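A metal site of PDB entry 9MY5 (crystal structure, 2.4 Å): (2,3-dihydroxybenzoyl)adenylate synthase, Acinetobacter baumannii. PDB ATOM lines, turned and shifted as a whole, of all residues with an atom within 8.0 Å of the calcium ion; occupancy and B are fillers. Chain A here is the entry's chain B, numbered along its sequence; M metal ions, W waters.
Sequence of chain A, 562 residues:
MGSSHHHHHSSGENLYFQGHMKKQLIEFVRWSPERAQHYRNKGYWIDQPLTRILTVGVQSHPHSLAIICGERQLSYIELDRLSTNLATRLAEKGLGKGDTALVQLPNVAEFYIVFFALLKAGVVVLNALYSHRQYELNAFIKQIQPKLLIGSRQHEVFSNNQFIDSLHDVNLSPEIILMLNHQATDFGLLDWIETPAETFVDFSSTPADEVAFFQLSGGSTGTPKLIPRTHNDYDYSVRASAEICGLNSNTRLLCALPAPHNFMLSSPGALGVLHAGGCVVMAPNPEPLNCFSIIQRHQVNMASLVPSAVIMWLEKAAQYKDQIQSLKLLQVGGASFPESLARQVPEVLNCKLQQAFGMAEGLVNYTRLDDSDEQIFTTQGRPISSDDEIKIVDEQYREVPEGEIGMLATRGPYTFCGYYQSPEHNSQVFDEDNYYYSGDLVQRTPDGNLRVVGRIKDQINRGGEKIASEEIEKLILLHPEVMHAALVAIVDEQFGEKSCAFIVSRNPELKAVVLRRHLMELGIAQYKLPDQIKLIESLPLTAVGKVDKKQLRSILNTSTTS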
ATOM      1  N   VAL A 300     -18.370  -2.283  19.813  1.00  0.00           N
ATOM      2  CA  VAL A 300     -17.281  -2.108  18.853  1.00  0.00           C
ATOM      3  C   VAL A 300     -17.356  -0.712  18.239  1.00  0.00           C
ATOM      4  O   VAL A 300     -18.444  -0.250  17.863  1.00  0.00           O
ATOM      5  CB  VAL A 300     -17.361  -3.211  17.775  1.00  0.00           C
ATOM      6  CG1 VAL A 300     -16.449  -2.878  16.623  1.00  0.00           C
ATOM      7  CG2 VAL A 300     -17.013  -4.567  18.389  1.00  0.00           C
ATOM      8  N   ASN A 301     -16.210  -0.018  18.153  1.00  0.00           N
ATOM      9  CA  ASN A 301     -16.230   1.295  17.530  1.00  0.00           C
ATOM     10  C   ASN A 301     -15.344   1.404  16.296  1.00  0.00           C
ATOM     11  O   ASN A 301     -15.255   2.486  15.715  1.00  0.00           O
ATOM     12  CB  ASN A 301     -15.869   2.406  18.540  1.00  0.00           C
ATOM     13  CG  ASN A 301     -14.598   2.124  19.292  1.00  0.00           C
ATOM     14  OD1 ASN A 301     -13.683   1.477  18.779  1.00  0.00           O
ATOM     15  ND2 ASN A 301     -14.521   2.619  20.524  1.00  0.00           N
ATOM     16  N   LYS A 321     -29.687  -0.669  12.155  1.00  0.00           N
ATOM     17  CA  LYS A 321     -29.058   0.581  12.558  1.00  0.00           C
ATOM     18  C   LYS A 321     -28.671   0.558  14.028  1.00  0.00           C
ATOM     19  O   LYS A 321     -27.550   0.948  14.380  1.00  0.00           O
ATOM     20  CB  LYS A 321     -29.961   1.774  12.277  1.00  0.00           C
ATOM     21  CG  LYS A 321     -29.810   2.367  10.893  1.00  0.00           C
ATOM     22  CD  LYS A 321     -31.001   3.265  10.571  1.00  0.00           C
ATOM     23  N   ILE A 324     -25.503  -1.431  15.214  1.00  0.00           N
ATOM     24  CA  ILE A 324     -24.200  -0.994  14.764  1.00  0.00           C
ATOM     25  C   ILE A 324     -23.952   0.491  15.032  1.00  0.00           C
ATOM     26  O   ILE A 324     -22.958   1.037  14.559  1.00  0.00           O
ATOM     27  CB  ILE A 324     -23.974  -1.341  13.277  1.00  0.00           C
ATOM     28  CG1 ILE A 324     -24.803  -0.443  12.372  1.00  0.00           C
ATOM     29  CG2 ILE A 324     -24.334  -2.792  12.998  1.00  0.00           C
ATOM     30  CD1 ILE A 324     -24.271  -0.441  10.972  1.00  0.00           C
ATOM     31  N   GLN A 325     -24.819   1.162  15.802  1.00  0.00           N
ATOM     32  CA  GLN A 325     -24.650   2.601  16.010  1.00  0.00           C
ATOM     33  C   GLN A 325     -23.258   2.949  16.552  1.00  0.00           C
ATOM     34  O   GLN A 325     -22.656   3.956  16.137  1.00  0.00           O
ATOM     35  CB  GLN A 325     -25.715   3.139  16.964  1.00  0.00           C
ATOM     36  CG  GLN A 325     -25.769   2.436  18.328  1.00  0.00           C
ATOM     37  CD  GLN A 325     -26.843   3.021  19.259  1.00  0.00           C
ATOM     38  OE1 GLN A 325     -27.015   2.562  20.411  1.00  0.00           O
ATOM     39  NE2 GLN A 325     -27.568   4.009  18.763  1.00  0.00           N
ATOM     40  N   SER A 326     -22.730   2.137  17.477  1.00  0.00           N
ATOM     41  CA  SER A 326     -21.465   2.467  18.144  1.00  0.00           C
ATOM     42  C   SER A 326     -20.282   2.465  17.191  1.00  0.00           C
ATOM     43  O   SER A 326     -19.194   2.947  17.573  1.00  0.00           O
ATOM     44  CB  SER A 326     -21.186   1.486  19.295  1.00  0.00           C
ATOM     45  OG  SER A 326     -20.780   0.227  18.780  1.00  0.00           O
ATOM     46  N   LEU A 327     -20.437   1.945  15.989  1.00  0.00           N
ATOM     47  CA  LEU A 327     -19.369   2.011  15.009  1.00  0.00           C
ATOM     48  C   LEU A 327     -18.988   3.462  14.757  1.00  0.00           C
ATOM     49  O   LEU A 327     -19.856   4.315  14.525  1.00  0.00           O
ATOM     50  CB  LEU A 327     -19.812   1.348  13.723  1.00  0.00           C
ATOM     51  CG  LEU A 327     -18.796   0.639  12.852  1.00  0.00           C
ATOM     52  CD1 LEU A 327     -17.883  -0.158  13.751  1.00  0.00           C
ATOM     53  CD2 LEU A 327     -19.563  -0.285  11.930  1.00  0.00           C
ATOM     54  N   LYS A 328     -17.686   3.763  14.849  1.00  0.00           N
ATOM     55  CA  LYS A 328     -17.189   5.109  14.622  1.00  0.00           C
ATOM     56  C   LYS A 328     -16.326   5.248  13.386  1.00  0.00           C
ATOM     57  O   LYS A 328     -16.248   6.340  12.822  1.00  0.00           O
ATOM     58  CB  LYS A 328     -16.389   5.577  15.841  1.00  0.00           C
ATOM     59  CG  LYS A 328     -17.224   6.075  16.993  1.00  0.00           C
ATOM     60  CD  LYS A 328     -16.354   6.854  18.000  1.00  0.00           C
ATOM     61  CE  LYS A 328     -16.876   6.571  19.395  1.00  0.00           C
ATOM     62  NZ  LYS A 328     -18.202   5.802  19.319  1.00  0.00           N
ATOM     63  N   LEU A 329     -15.658   4.184  12.956  1.00  0.00           N
ATOM     64  CA  LEU A 329     -14.673   4.324  11.901  1.00  0.00           C
ATOM     65  C   LEU A 329     -14.510   2.995  11.173  1.00  0.00           C
ATOM     66  O   LEU A 329     -14.343   1.955  11.819  1.00  0.00           O
ATOM     67  CB  LEU A 329     -13.319   4.808  12.479  1.00  0.00           C
ATOM     68  CG  LEU A 329     -12.140   4.812  11.514  1.00  0.00           C
ATOM     69  CD1 LEU A 329     -12.420   5.793  10.363  1.00  0.00           C
ATOM     70  CD2 LEU A 329     -10.781   5.131  12.201  1.00  0.00           C
ATOM     71  N   PRO A 346     -20.811   6.310   5.272  1.00  0.00           N
ATOM     72  CA  PRO A 346     -21.377   7.241   6.251  1.00  0.00           C
ATOM     73  C   PRO A 346     -22.889   7.292   6.234  1.00  0.00           C
ATOM     74  O   PRO A 346     -23.497   7.436   7.305  1.00  0.00           O
ATOM     75  CB  PRO A 346     -20.742   8.593   5.866  1.00  0.00           C
ATOM     76  CG  PRO A 346     -20.163   8.412   4.510  1.00  0.00           C
ATOM     77  CD  PRO A 346     -19.877   6.956   4.335  1.00  0.00           C
ATOM     78  N   LEU A 349     -24.039   2.907   7.060  1.00  0.00           N
ATOM     79  CA  LEU A 349     -23.377   2.348   8.232  1.00  0.00           C
ATOM     80  C   LEU A 349     -23.142   3.367   9.347  1.00  0.00           C
ATOM     81  O   LEU A 349     -22.749   2.974  10.452  1.00  0.00           O
ATOM     82  CB  LEU A 349     -22.053   1.698   7.839  1.00  0.00           C
ATOM     83  CG  LEU A 349     -22.129   0.566   6.812  1.00  0.00           C
ATOM     84  CD1 LEU A 349     -20.705   0.117   6.424  1.00  0.00           C
ATOM     85  CD2 LEU A 349     -22.957  -0.581   7.361  1.00  0.00           C
ATOM     86  N   ASN A 350     -23.383   4.649   9.088  1.00  0.00           N
ATOM     87  CA  ASN A 350     -23.386   5.688  10.131  1.00  0.00           C
ATOM     88  C   ASN A 350     -22.035   5.755  10.857  1.00  0.00           C
ATOM     89  O   ASN A 350     -21.954   5.821  12.098  1.00  0.00           O
ATOM     90  CB  ASN A 350     -24.544   5.462  11.107  1.00  0.00           C
ATOM     91  CG  ASN A 350     -25.899   5.543  10.420  1.00  0.00           C
ATOM     92  OD1 ASN A 350     -26.049   6.243   9.428  1.00  0.00           O
ATOM     93  ND2 ASN A 350     -26.887   4.818  10.945  1.00  0.00           N
ATOM     94  N   CYS A 351     -20.957   5.785  10.086  1.00  0.00           N
ATOM     95  CA  CYS A 351     -19.634   5.954  10.648  1.00  0.00           C
ATOM     96  C   CYS A 351     -18.722   6.585   9.597  1.00  0.00           C
ATOM     97  O   CYS A 351     -18.991   6.493   8.392  1.00  0.00           O
ATOM     98  CB  CYS A 351     -19.060   4.621  11.114  1.00  0.00           C
ATOM     99  SG  CYS A 351     -18.809   3.537   9.686  1.00  0.00           S
ATOM    100  N   LYS A 352     -17.639   7.192  10.056  1.00  0.00           N
ATOM    101  CA  LYS A 352     -16.644   7.753   9.155  1.00  0.00           C
ATOM    102  C   LYS A 352     -16.024   6.654   8.283  1.00  0.00           C
ATOM    103  O   LYS A 352     -15.915   5.500   8.689  1.00  0.00           O
ATOM    104  CB  LYS A 352     -15.533   8.457   9.938  1.00  0.00           C
ATOM    105  CG  LYS A 352     -14.474   9.103   9.064  1.00  0.00           C
ATOM    106  CD  LYS A 352     -14.003  10.455   9.619  1.00  0.00           C
ATOM    107  CE  LYS A 352     -13.322  11.325   8.530  1.00  0.00           C
ATOM    108  NZ  LYS A 352     -13.969  12.678   8.345  1.00  0.00           N
HETATM  109 CA    CA M   1     -21.816   5.283  14.416  1.00  0.00          CA
HETATM  110  O   HOH W   1     -22.758   3.361  13.375  1.00  0.00           O
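Of the 14 residues printed, 3 come within 4 Å of the calcium ion.
Along chain A the residues within 4 Å of the calcium ion span positions 325 to 350.
The nearest printed residue that does not touch the calcium ion is Ser 326 (4.2 Å).
The calcium ion is bound by O of Leu 327 (2.2 Å), O of Gln 325 (2.3 Å), water W1 (2.4 Å) and O of Asn 350 (2.4 Å).
The calcium ion has four donor atoms within binding distance.
Water W1 lies within hydrogen-bond range of O of Ile 324 and O of Leu 349.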
